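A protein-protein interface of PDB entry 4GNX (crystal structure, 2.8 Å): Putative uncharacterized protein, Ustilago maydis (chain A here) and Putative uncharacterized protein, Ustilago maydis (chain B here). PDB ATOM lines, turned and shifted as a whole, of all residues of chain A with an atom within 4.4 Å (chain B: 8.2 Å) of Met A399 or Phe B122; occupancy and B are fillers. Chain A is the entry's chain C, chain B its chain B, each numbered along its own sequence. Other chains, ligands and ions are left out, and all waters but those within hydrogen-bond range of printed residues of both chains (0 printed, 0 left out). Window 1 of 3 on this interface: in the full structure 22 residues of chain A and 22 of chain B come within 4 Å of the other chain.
The guanidinium group (NE) of Arg B92 is in hydrogen-bond range of the side-chain hydroxyl (OG1) of Thr B40 (2.8 Å). N of Arg B92 lies within hydrogen-bond range of O of Arg B112, at 2.8 Å. The guanidinium group (NH1) of Arg B92 is in salt-bridge range of the side-chain carboxylate (OE2) of Glu B119, 2.4 Å away. NH2 of Arg B92 lies within salt-bridge range of OE2 of Glu B126, 3.7 Å away. The side-chain carboxylate of Glu B119 lies within salt-bridge range of the guanidinium group of Arg B112, at 2.9 Å. N of Val A427 sits at hydrogen-bond distance from O of Met A399 (3.3 Å).
Arg A295 touches Phe B122. CB of Thr A297 touches CD2 of Leu B9 (3.8 Å). NH2 of Arg B92 touches CE of Met A399, 3.6 Å away. CE2 of Phe B122 touches SD of Met A399, 3.9 Å away. CE1 of Phe A429 touches CD1 of Ile B115 (3.7 Å). CD of Glu B119 touches CZ of Phe A429 (3.3 Å). CD1 of Phe B122 touches N of Gly A433, at 3.9 Å. Gly A433 touches Leu B125. Glu B126 touches Leu A436 (N to CD1, 3.9 Å). CD2 of Leu A436 touches CB of His B129, at 3.5 Å.
Printed residues of chain B within 4 Å of Arg A295: Phe B122. Printed residues of chain B within 4 Å of Thr A297: Leu B9. Printed residues of chain B within 4 Å of Met A399: Arg B92 and Phe B122. Of the printed residues of chain A, Ile B115 touches Phe A429 (3.7 Å). Of the printed residues of chain A, Glu B126 touches Leu A436. The nearest printed residue of chain B that does not touch Met A399 is Arg B112 (4.4 Å).
Hydrophobic or aromatic side chains of chain B within 4 Å of the printed part of chain A: Leu B9, Ile B115, Phe B122, Leu B125 and His B129. Hydrophobic or aromatic side chains of chain A within 4 Å of the printed part of chain B: Met A399, Phe A429, Ala A432 and Leu A436. Among the printed residues, 17 pairs touch across the chains. Among the printed residues, no Asp or Glu carboxylate lies within 4 Å of a Lys or Arg side-chain nitrogen of the other chain.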
ATOM      1  N   ARG A 295       9.248  -3.276 -12.739  1.00  0.00           N
ATOM      2  CA  ARG A 295       8.989  -3.079 -14.160  1.00  0.00           C
ATOM      3  C   ARG A 295      10.009  -2.046 -14.615  1.00  0.00           C
ATOM      4  O   ARG A 295      10.007  -0.924 -14.101  1.00  0.00           O
ATOM      5  CB  ARG A 295       7.586  -2.522 -14.369  1.00  0.00           C
ATOM      6  CG  ARG A 295       6.978  -2.902 -15.698  1.00  0.00           C
ATOM      7  CD  ARG A 295       5.745  -2.091 -16.096  1.00  0.00           C
ATOM      8  NE  ARG A 295       4.638  -2.023 -15.132  1.00  0.00           N
ATOM      9  CZ  ARG A 295       3.873  -3.048 -14.762  1.00  0.00           C
ATOM     10  NH1 ARG A 295       4.091  -4.278 -15.216  1.00  0.00           N
ATOM     11  NH2 ARG A 295       2.886  -2.843 -13.907  1.00  0.00           N
ATOM     12  N   ALA A 296      10.897  -2.410 -15.537  1.00  0.00           N
ATOM     13  CA  ALA A 296      11.873  -1.454 -16.063  1.00  0.00           C
ATOM     14  C   ALA A 296      12.229  -1.723 -17.507  1.00  0.00           C
ATOM     15  O   ALA A 296      11.936  -2.808 -18.036  1.00  0.00           O
ATOM     16  CB  ALA A 296      13.119  -1.423 -15.207  1.00  0.00           C
ATOM     17  N   THR A 297      12.846  -0.732 -18.145  1.00  0.00           N
ATOM     18  CA  THR A 297      13.197  -0.835 -19.549  1.00  0.00           C
ATOM     19  C   THR A 297      14.691  -0.975 -19.657  1.00  0.00           C
ATOM     20  O   THR A 297      15.431  -0.214 -19.021  1.00  0.00           O
ATOM     21  CB  THR A 297      12.785   0.416 -20.333  1.00  0.00           C
ATOM     22  OG1 THR A 297      11.362   0.577 -20.261  1.00  0.00           O
ATOM     23  CG2 THR A 297      13.191   0.296 -21.767  1.00  0.00           C
ATOM     24  N   ARG A 398      13.497  -2.371 -24.484  1.00  0.00           N
ATOM     25  CA  ARG A 398      12.538  -3.450 -24.231  1.00  0.00           C
ATOM     26  C   ARG A 398      12.219  -3.505 -22.760  1.00  0.00           C
ATOM     27  O   ARG A 398      13.093  -3.241 -21.929  1.00  0.00           O
ATOM     28  CB  ARG A 398      13.088  -4.801 -24.668  1.00  0.00           C
ATOM     29  CG  ARG A 398      13.377  -4.912 -26.136  1.00  0.00           C
ATOM     30  CD  ARG A 398      12.806  -6.219 -26.649  1.00  0.00           C
ATOM     31  NE  ARG A 398      13.466  -6.597 -27.886  1.00  0.00           N
ATOM     32  CZ  ARG A 398      12.906  -6.520 -29.077  1.00  0.00           C
ATOM     33  NH1 ARG A 398      11.653  -6.099 -29.192  1.00  0.00           N
ATOM     34  NH2 ARG A 398      13.597  -6.883 -30.148  1.00  0.00           N
ATOM     35  N   MET A 399      10.981  -3.874 -22.444  1.00  0.00           N
ATOM     36  CA  MET A 399      10.443  -3.750 -21.089  1.00  0.00           C
ATOM     37  C   MET A 399      10.209  -5.089 -20.385  1.00  0.00           C
ATOM     38  O   MET A 399       9.623  -6.021 -20.957  1.00  0.00           O
ATOM     39  CB  MET A 399       9.141  -2.965 -21.149  1.00  0.00           C
ATOM     40  CG  MET A 399       8.791  -2.258 -19.858  1.00  0.00           C
ATOM     41  SD  MET A 399       7.435  -1.084 -20.040  1.00  0.00           S
ATOM     42  CE  MET A 399       7.945  -0.192 -21.526  1.00  0.00           C
ATOM     43  N   TYR A 400      10.643  -5.179 -19.128  1.00  0.00           N
ATOM     44  CA  TYR A 400      10.547  -6.452 -18.397  1.00  0.00           C
ATOM     45  C   TYR A 400      10.069  -6.307 -16.981  1.00  0.00           C
ATOM     46  O   TYR A 400      10.322  -5.291 -16.342  1.00  0.00           O
ATOM     47  CB  TYR A 400      11.911  -7.168 -18.339  1.00  0.00           C
ATOM     48  CG  TYR A 400      12.460  -7.538 -19.678  1.00  0.00           C
ATOM     49  CD1 TYR A 400      13.199  -6.634 -20.424  1.00  0.00           C
ATOM     50  CD2 TYR A 400      12.215  -8.777 -20.204  1.00  0.00           C
ATOM     51  CE1 TYR A 400      13.683  -6.965 -21.664  1.00  0.00           C
ATOM     52  CE2 TYR A 400      12.696  -9.128 -21.445  1.00  0.00           C
ATOM     53  CZ  TYR A 400      13.430  -8.220 -22.168  1.00  0.00           C
ATOM     54  OH  TYR A 400      13.909  -8.596 -23.399  1.00  0.00           O
ATOM     55  N   PRO A 426       8.980 -10.882 -19.850  1.00  0.00           N
ATOM     56  CA  PRO A 426       8.565  -9.747 -20.689  1.00  0.00           C
ATOM     57  C   PRO A 426       7.205  -9.237 -20.213  1.00  0.00           C
ATOM     58  O   PRO A 426       6.354 -10.030 -19.837  1.00  0.00           O
ATOM     59  CB  PRO A 426       8.462 -10.368 -22.077  1.00  0.00           C
ATOM     60  CG  PRO A 426       8.124 -11.800 -21.806  1.00  0.00           C
ATOM     61  CD  PRO A 426       8.869 -12.171 -20.560  1.00  0.00           C
ATOM     62  N   VAL A 427       7.016  -7.929 -20.199  1.00  0.00           N
ATOM     63  CA  VAL A 427       5.761  -7.349 -19.712  1.00  0.00           C
ATOM     64  C   VAL A 427       4.510  -7.843 -20.449  1.00  0.00           C
ATOM     65  O   VAL A 427       4.479  -7.896 -21.687  1.00  0.00           O
ATOM     66  CB  VAL A 427       5.801  -5.809 -19.784  1.00  0.00           C
ATOM     67  CG1 VAL A 427       4.437  -5.215 -19.427  1.00  0.00           C
ATOM     68  CG2 VAL A 427       6.916  -5.246 -18.890  1.00  0.00           C
ATOM     69  N   PHE A 429       1.305  -6.601 -21.461  1.00  0.00           N
ATOM     70  CA  PHE A 429       0.761  -5.257 -21.604  1.00  0.00           C
ATOM     71  C   PHE A 429      -0.679  -5.120 -21.187  1.00  0.00           C
ATOM     72  O   PHE A 429      -1.014  -4.181 -20.476  1.00  0.00           O
ATOM     73  CB  PHE A 429       0.994  -4.713 -23.014  1.00  0.00           C
ATOM     74  CG  PHE A 429       2.423  -4.338 -23.263  1.00  0.00           C
ATOM     75  CD1 PHE A 429       3.155  -4.952 -24.272  1.00  0.00           C
ATOM     76  CD2 PHE A 429       3.046  -3.394 -22.448  1.00  0.00           C
ATOM     77  CE1 PHE A 429       4.471  -4.603 -24.487  1.00  0.00           C
ATOM     78  CE2 PHE A 429       4.371  -3.051 -22.642  1.00  0.00           C
ATOM     79  CZ  PHE A 429       5.084  -3.659 -23.665  1.00  0.00           C
ATOM     80  N   ALA A 432      -0.601  -5.591 -17.214  1.00  0.00           N
ATOM     81  CA  ALA A 432       0.032  -4.370 -16.670  1.00  0.00           C
ATOM     82  C   ALA A 432      -0.890  -3.152 -16.867  1.00  0.00           C
ATOM     83  O   ALA A 432      -0.964  -2.265 -16.013  1.00  0.00           O
ATOM     84  CB  ALA A 432       1.375  -4.115 -17.312  1.00  0.00           C
ATOM     85  N   GLY A 433      -1.607  -3.138 -17.989  1.00  0.00           N
ATOM     86  CA  GLY A 433      -2.606  -2.124 -18.267  1.00  0.00           C
ATOM     87  C   GLY A 433      -3.719  -2.037 -17.245  1.00  0.00           C
ATOM     88  O   GLY A 433      -3.989  -0.959 -16.712  1.00  0.00           O
ATOM     89  N   LEU A 436      -2.581  -0.559 -13.993  1.00  0.00           N
ATOM     90  CA  LEU A 436      -2.557   0.885 -14.125  1.00  0.00           C
ATOM     91  C   LEU A 436      -3.936   1.546 -14.090  1.00  0.00           C
ATOM     92  O   LEU A 436      -4.078   2.624 -13.505  1.00  0.00           O
ATOM     93  CB  LEU A 436      -1.817   1.307 -15.398  1.00  0.00           C
ATOM     94  CG  LEU A 436      -0.284   1.309 -15.349  1.00  0.00           C
ATOM     95  CD1 LEU A 436       0.372   1.468 -16.718  1.00  0.00           C
ATOM     96  CD2 LEU A 436       0.109   2.436 -14.434  1.00  0.00           C
ATOM     97  N   LEU B   9      13.637   7.969 -16.842  1.00  0.00           N
ATOM     98  CA  LEU B   9      13.075   7.655 -18.138  1.00  0.00           C
ATOM     99  C   LEU B   9      11.565   7.820 -18.069  1.00  0.00           C
ATOM    100  O   LEU B   9      10.840   6.926 -17.631  1.00  0.00           O
ATOM    101  CB  LEU B   9      13.434   6.227 -18.565  1.00  0.00           C
ATOM    102  CG  LEU B   9      12.725   5.748 -19.841  1.00  0.00           C
ATOM    103  CD1 LEU B   9      13.271   6.493 -21.047  1.00  0.00           C
ATOM    104  CD2 LEU B   9      12.794   4.233 -20.018  1.00  0.00           C
ATOM    105  N   PRO B  11       7.710   8.287 -19.161  1.00  0.00           N
ATOM    106  CA  PRO B  11       6.746   8.047 -20.212  1.00  0.00           C
ATOM    107  C   PRO B  11       5.897   9.338 -20.423  1.00  0.00           C
ATOM    108  O   PRO B  11       5.421   9.945 -19.469  1.00  0.00           O
ATOM    109  CB  PRO B  11       5.920   6.895 -19.634  1.00  0.00           C
ATOM    110  CG  PRO B  11       5.915   7.160 -18.143  1.00  0.00           C
ATOM    111  CD  PRO B  11       7.259   7.762 -17.850  1.00  0.00           C
ATOM    112  N   THR B  40      10.226   8.352 -23.121  1.00  0.00           N
ATOM    113  CA  THR B  40       9.752   7.335 -24.032  1.00  0.00           C
ATOM    114  C   THR B  40       8.277   7.475 -24.397  1.00  0.00           C
ATOM    115  O   THR B  40       7.452   7.949 -23.609  1.00  0.00           O
ATOM    116  CB  THR B  40       9.970   5.923 -23.475  1.00  0.00           C
ATOM    117  OG1 THR B  40       9.464   4.982 -24.431  1.00  0.00           O
ATOM    118  CG2 THR B  40       9.255   5.720 -22.110  1.00  0.00           C
ATOM    119  N   VAL B  42       5.005   6.080 -27.573  1.00  0.00           N
ATOM    120  CA  VAL B  42       4.570   5.204 -28.652  1.00  0.00           C
ATOM    121  C   VAL B  42       3.803   6.067 -29.627  1.00  0.00           C
ATOM    122  O   VAL B  42       3.064   6.950 -29.224  1.00  0.00           O
ATOM    123  CB  VAL B  42       3.676   4.091 -28.112  1.00  0.00           C
ATOM    124  CG1 VAL B  42       3.069   3.298 -29.251  1.00  0.00           C
ATOM    125  CG2 VAL B  42       4.468   3.174 -27.185  1.00  0.00           C
ATOM    126  N   ARG B  92       7.743   2.126 -30.552  1.00  0.00           N
ATOM    127  CA  ARG B  92       8.184   2.555 -29.224  1.00  0.00           C
ATOM    128  C   ARG B  92       9.413   3.433 -29.470  1.00  0.00           C
ATOM    129  O   ARG B  92      10.351   3.033 -30.164  1.00  0.00           O
ATOM    130  CB  ARG B  92       8.480   1.309 -28.344  1.00  0.00           C
ATOM    131  CG  ARG B  92       8.748   1.451 -26.830  1.00  0.00           C
ATOM    132  CD  ARG B  92       8.394   2.798 -26.255  1.00  0.00           C
ATOM    133  NE  ARG B  92       7.749   2.883 -24.924  1.00  0.00           N
ATOM    134  CZ  ARG B  92       6.719   2.159 -24.499  1.00  0.00           C
ATOM    135  NH1 ARG B  92       6.256   1.186 -25.255  1.00  0.00           N
ATOM    136  NH2 ARG B  92       6.164   2.402 -23.308  1.00  0.00           N
ATOM    137  N   LEU B  94      12.529   5.639 -27.791  1.00  0.00           N
ATOM    138  CA  LEU B  94      13.333   6.036 -26.646  1.00  0.00           C
ATOM    139  C   LEU B  94      14.279   7.153 -27.098  1.00  0.00           C
ATOM    140  O   LEU B  94      14.916   7.028 -28.152  1.00  0.00           O
ATOM    141  CB  LEU B  94      14.111   4.831 -26.131  1.00  0.00           C
ATOM    142  CG  LEU B  94      14.635   4.978 -24.711  1.00  0.00           C
ATOM    143  CD1 LEU B  94      14.569   3.668 -23.948  1.00  0.00           C
ATOM    144  CD2 LEU B  94      16.055   5.480 -24.758  1.00  0.00           C
ATOM    145  N   ARG B 112      11.603   0.886 -31.953  1.00  0.00           N
ATOM    146  CA  ARG B 112      11.158  -0.460 -32.273  1.00  0.00           C
ATOM    147  C   ARG B 112       9.656  -0.593 -32.613  1.00  0.00           C
ATOM    148  O   ARG B 112       8.794  -0.004 -31.948  1.00  0.00           O
ATOM    149  CB  ARG B 112      11.535  -1.360 -31.110  1.00  0.00           C
ATOM    150  CG  ARG B 112      10.580  -2.504 -30.873  1.00  0.00           C
ATOM    151  CD  ARG B 112      10.668  -2.973 -29.439  1.00  0.00           C
ATOM    152  NE  ARG B 112       9.786  -2.218 -28.568  1.00  0.00           N
ATOM    153  CZ  ARG B 112       9.601  -2.519 -27.294  1.00  0.00           C
ATOM    154  NH1 ARG B 112      10.245  -3.552 -26.770  1.00  0.00           N
ATOM    155  NH2 ARG B 112       8.787  -1.803 -26.544  1.00  0.00           N
ATOM    156  N   ILE B 115       5.021  -4.173 -30.084  1.00  0.00           N
ATOM    157  CA  ILE B 115       4.826  -5.614 -29.899  1.00  0.00           C
ATOM    158  C   ILE B 115       3.404  -6.053 -30.307  1.00  0.00           C
ATOM    159  O   ILE B 115       3.222  -6.867 -31.243  1.00  0.00           O
ATOM    160  CB  ILE B 115       5.165  -6.073 -28.434  1.00  0.00           C
ATOM    161  CG1 ILE B 115       6.523  -5.510 -27.962  1.00  0.00           C
ATOM    162  CG2 ILE B 115       5.160  -7.599 -28.327  1.00  0.00           C
ATOM    163  CD1 ILE B 115       7.042  -6.067 -26.642  1.00  0.00           C
ATOM    164  N   ASP B 116       2.428  -5.513 -29.576  1.00  0.00           N
ATOM    165  CA  ASP B 116       1.013  -5.675 -29.836  1.00  0.00           C
ATOM    166  C   ASP B 116       0.349  -4.320 -29.548  1.00  0.00           C
ATOM    167  O   ASP B 116       0.972  -3.413 -28.983  1.00  0.00           O
ATOM    168  CB  ASP B 116       0.437  -6.788 -28.951  1.00  0.00           C
ATOM    169  CG  ASP B 116       0.585  -6.509 -27.451  1.00  0.00           C
ATOM    170  OD1 ASP B 116       0.091  -7.309 -26.614  1.00  0.00           O
ATOM    171  OD2 ASP B 116       1.189  -5.484 -27.091  1.00  0.00           O
ATOM    172  N   TYR B 117      -0.908  -4.183 -29.941  1.00  0.00           N
ATOM    173  CA  TYR B 117      -1.641  -2.939 -29.752  1.00  0.00           C
ATOM    174  C   TYR B 117      -1.845  -2.587 -28.286  1.00  0.00           C
ATOM    175  O   TYR B 117      -1.878  -1.412 -27.936  1.00  0.00           O
ATOM    176  CB  TYR B 117      -2.996  -2.995 -30.456  1.00  0.00           C
ATOM    177  CG  TYR B 117      -3.666  -1.674 -30.466  1.00  0.00           C
ATOM    178  CD1 TYR B 117      -3.229  -0.671 -31.324  1.00  0.00           C
ATOM    179  CD2 TYR B 117      -4.702  -1.398 -29.590  1.00  0.00           C
ATOM    180  CE1 TYR B 117      -3.819   0.575 -31.327  1.00  0.00           C
ATOM    181  CE2 TYR B 117      -5.305  -0.160 -29.580  1.00  0.00           C
ATOM    182  CZ  TYR B 117      -4.862   0.830 -30.458  1.00  0.00           C
ATOM    183  OH  TYR B 117      -5.438   2.092 -30.480  1.00  0.00           O
ATOM    184  N   ASN B 118      -1.984  -3.593 -27.432  1.00  0.00           N
ATOM    185  CA  ASN B 118      -2.113  -3.349 -26.013  1.00  0.00           C
ATOM    186  C   ASN B 118      -0.988  -2.498 -25.457  1.00  0.00           C
ATOM    187  O   ASN B 118      -1.194  -1.785 -24.479  1.00  0.00           O
ATOM    188  CB  ASN B 118      -2.168  -4.651 -25.239  1.00  0.00           C
ATOM    189  CG  ASN B 118      -3.420  -5.441 -25.511  1.00  0.00           C
ATOM    190  OD1 ASN B 118      -4.525  -4.976 -25.240  1.00  0.00           O
ATOM    191  ND2 ASN B 118      -3.258  -6.654 -26.022  1.00  0.00           N
ATOM    192  N   GLU B 119       0.202  -2.564 -26.044  1.00  0.00           N
ATOM    193  CA  GLU B 119       1.271  -1.709 -25.577  1.00  0.00           C
ATOM    194  C   GLU B 119       0.945  -0.228 -25.761  1.00  0.00           C
ATOM    195  O   GLU B 119       1.222   0.596 -24.867  1.00  0.00           O
ATOM    196  CB  GLU B 119       2.575  -2.030 -26.272  1.00  0.00           C
ATOM    197  CG  GLU B 119       3.746  -1.244 -25.684  1.00  0.00           C
ATOM    198  CD  GLU B 119       5.100  -1.616 -26.278  1.00  0.00           C
ATOM    199  OE1 GLU B 119       5.171  -2.296 -27.337  1.00  0.00           O
ATOM    200  OE2 GLU B 119       6.112  -1.217 -25.674  1.00  0.00           O
ATOM    201  N   VAL B 120       0.368   0.112 -26.917  1.00  0.00           N
ATOM    202  CA  VAL B 120      -0.090   1.472 -27.189  1.00  0.00           C
ATOM    203  C   VAL B 120      -1.035   1.939 -26.073  1.00  0.00           C
ATOM    204  O   VAL B 120      -0.933   3.065 -25.554  1.00  0.00           O
ATOM    205  CB  VAL B 120      -0.846   1.549 -28.504  1.00  0.00           C
ATOM    206  CG1 VAL B 120      -1.143   2.996 -28.834  1.00  0.00           C
ATOM    207  CG2 VAL B 120      -0.059   0.892 -29.637  1.00  0.00           C
ATOM    208  N   MET B 121      -1.940   1.053 -25.675  1.00  0.00           N
ATOM    209  CA  MET B 121      -2.866   1.374 -24.612  1.00  0.00           C
ATOM    210  C   MET B 121      -2.140   1.508 -23.295  1.00  0.00           C
ATOM    211  O   MET B 121      -2.340   2.472 -22.574  1.00  0.00           O
ATOM    212  CB  MET B 121      -3.982   0.338 -24.551  1.00  0.00           C
ATOM    213  CG  MET B 121      -4.755   0.252 -25.858  1.00  0.00           C
ATOM    214  SD  MET B 121      -5.682   1.774 -26.159  1.00  0.00           S
ATOM    215  CE  MET B 121      -4.704   2.702 -27.338  1.00  0.00           C
ATOM    216  N   PHE B 122      -1.283   0.546 -22.986  1.00  0.00           N
ATOM    217  CA  PHE B 122      -0.490   0.563 -21.750  1.00  0.00           C
ATOM    218  C   PHE B 122       0.279   1.850 -21.632  1.00  0.00           C
ATOM    219  O   PHE B 122       0.362   2.450 -20.568  1.00  0.00           O
ATOM    220  CB  PHE B 122       0.497  -0.595 -21.767  1.00  0.00           C
ATOM    221  CG  PHE B 122       1.569  -0.495 -20.732  1.00  0.00           C
ATOM    222  CD1 PHE B 122       1.380  -1.041 -19.455  1.00  0.00           C
ATOM    223  CD2 PHE B 122       2.777   0.107 -21.031  1.00  0.00           C
ATOM    224  CE1 PHE B 122       2.374  -0.966 -18.496  1.00  0.00           C
ATOM    225  CE2 PHE B 122       3.769   0.176 -20.070  1.00  0.00           C
ATOM    226  CZ  PHE B 122       3.564  -0.356 -18.806  1.00  0.00           C
ATOM    227  N   HIS B 123       0.833   2.290 -22.750  1.00  0.00           N
ATOM    228  CA  HIS B 123       1.591   3.525 -22.724  1.00  0.00           C
ATOM    229  C   HIS B 123       0.845   4.805 -22.336  1.00  0.00           C
ATOM    230  O   HIS B 123       1.424   5.671 -21.655  1.00  0.00           O
ATOM    231  CB  HIS B 123       2.330   3.758 -24.018  1.00  0.00           C
ATOM    232  CG  HIS B 123       3.021   5.057 -24.014  1.00  0.00           C
ATOM    233  ND1 HIS B 123       3.972   5.344 -23.096  1.00  0.00           N
ATOM    234  CD2 HIS B 123       2.817   6.206 -24.752  1.00  0.00           C
ATOM    235  CE1 HIS B 123       4.403   6.611 -23.279  1.00  0.00           C
ATOM    236  NE2 HIS B 123       3.702   7.138 -24.292  1.00  0.00           N
ATOM    237  N   ARG B 124      -0.405   4.970 -22.786  1.00  0.00           N
ATOM    238  CA  ARG B 124      -1.155   6.155 -22.407  1.00  0.00           C
ATOM    239  C   ARG B 124      -1.340   6.189 -20.898  1.00  0.00           C
ATOM    240  O   ARG B 124      -1.211   7.249 -20.254  1.00  0.00           O
ATOM    241  CB  ARG B 124      -2.508   6.176 -23.076  1.00  0.00           C
ATOM    242  CG  ARG B 124      -2.452   6.552 -24.540  1.00  0.00           C
ATOM    243  CD  ARG B 124      -3.804   6.990 -25.039  1.00  0.00           C
ATOM    244  NE  ARG B 124      -3.636   7.818 -26.230  1.00  0.00           N
ATOM    245  CZ  ARG B 124      -4.535   8.684 -26.695  1.00  0.00           C
ATOM    246  NH1 ARG B 124      -5.690   8.861 -26.067  1.00  0.00           N
ATOM    247  NH2 ARG B 124      -4.260   9.377 -27.792  1.00  0.00           N
ATOM    248  N   LEU B 125      -1.605   5.015 -20.331  1.00  0.00           N
ATOM    249  CA  LEU B 125      -1.849   4.894 -18.901  1.00  0.00           C
ATOM    250  C   LEU B 125      -0.588   5.166 -18.118  1.00  0.00           C
ATOM    251  O   LEU B 125      -0.628   5.681 -17.002  1.00  0.00           O
ATOM    252  CB  LEU B 125      -2.416   3.521 -18.559  1.00  0.00           C
ATOM    253  CG  LEU B 125      -3.777   3.206 -19.197  1.00  0.00           C
ATOM    254  CD1 LEU B 125      -4.239   1.801 -18.855  1.00  0.00           C
ATOM    255  CD2 LEU B 125      -4.841   4.215 -18.785  1.00  0.00           C
ATOM    256  N   GLU B 126       0.545   4.825 -18.704  1.00  0.00           N
ATOM    257  CA  GLU B 126       1.784   4.957 -17.987  1.00  0.00           C
ATOM    258  C   GLU B 126       2.097   6.434 -17.861  1.00  0.00           C
ATOM    259  O   GLU B 126       2.551   6.887 -16.813  1.00  0.00           O
ATOM    260  CB  GLU B 126       2.886   4.202 -18.713  1.00  0.00           C
ATOM    261  CG  GLU B 126       3.939   3.634 -17.771  1.00  0.00           C
ATOM    262  CD  GLU B 126       5.116   2.976 -18.482  1.00  0.00           C
ATOM    263  OE1 GLU B 126       5.938   2.370 -17.736  1.00  0.00           O
ATOM    264  OE2 GLU B 126       5.217   3.068 -19.753  1.00  0.00           O
ATOM    265  N   ALA B 127       1.796   7.187 -18.923  1.00  0.00           N
ATOM    266  CA  ALA B 127       1.948   8.649 -18.931  1.00  0.00           C
ATOM    267  C   ALA B 127       1.024   9.305 -17.940  1.00  0.00           C
ATOM    268  O   ALA B 127       1.426  10.218 -17.226  1.00  0.00           O
ATOM    269  CB  ALA B 127       1.691   9.218 -20.306  1.00  0.00           C
ATOM    270  N   VAL B 128      -0.220   8.848 -17.893  1.00  0.00           N
ATOM    271  CA  VAL B 128      -1.158   9.368 -16.893  1.00  0.00           C
ATOM    272  C   VAL B 128      -0.572   9.074 -15.512  1.00  0.00           C
ATOM    273  O   VAL B 128      -0.332   9.992 -14.694  1.00  0.00           O
ATOM    274  CB  VAL B 128      -2.586   8.788 -17.071  1.00  0.00           C
ATOM    275  CG1 VAL B 128      -3.515   9.239 -15.962  1.00  0.00           C
ATOM    276  CG2 VAL B 128      -3.161   9.226 -18.411  1.00  0.00           C
ATOM    277  N   HIS B 129      -0.300   7.801 -15.264  1.00  0.00           N
ATOM    278  CA  HIS B 129       0.202   7.392 -13.960  1.00  0.00           C
ATOM    279  C   HIS B 129       1.427   8.160 -13.553  1.00  0.00           C
ATOM    280  O   HIS B 129       1.512   8.654 -12.429  1.00  0.00           O
ATOM    281  CB  HIS B 129       0.452   5.884 -13.915  1.00  0.00           C
ATOM    282  CG  HIS B 129       0.846   5.391 -12.559  1.00  0.00           C
ATOM    283  ND1 HIS B 129      -0.024   5.320 -11.541  1.00  0.00           N
ATOM    284  CD2 HIS B 129       2.070   5.002 -12.059  1.00  0.00           C
ATOM    285  CE1 HIS B 129       0.604   4.890 -10.437  1.00  0.00           C
ATOM    286  NE2 HIS B 129       1.887   4.703 -10.748  1.00  0.00           N
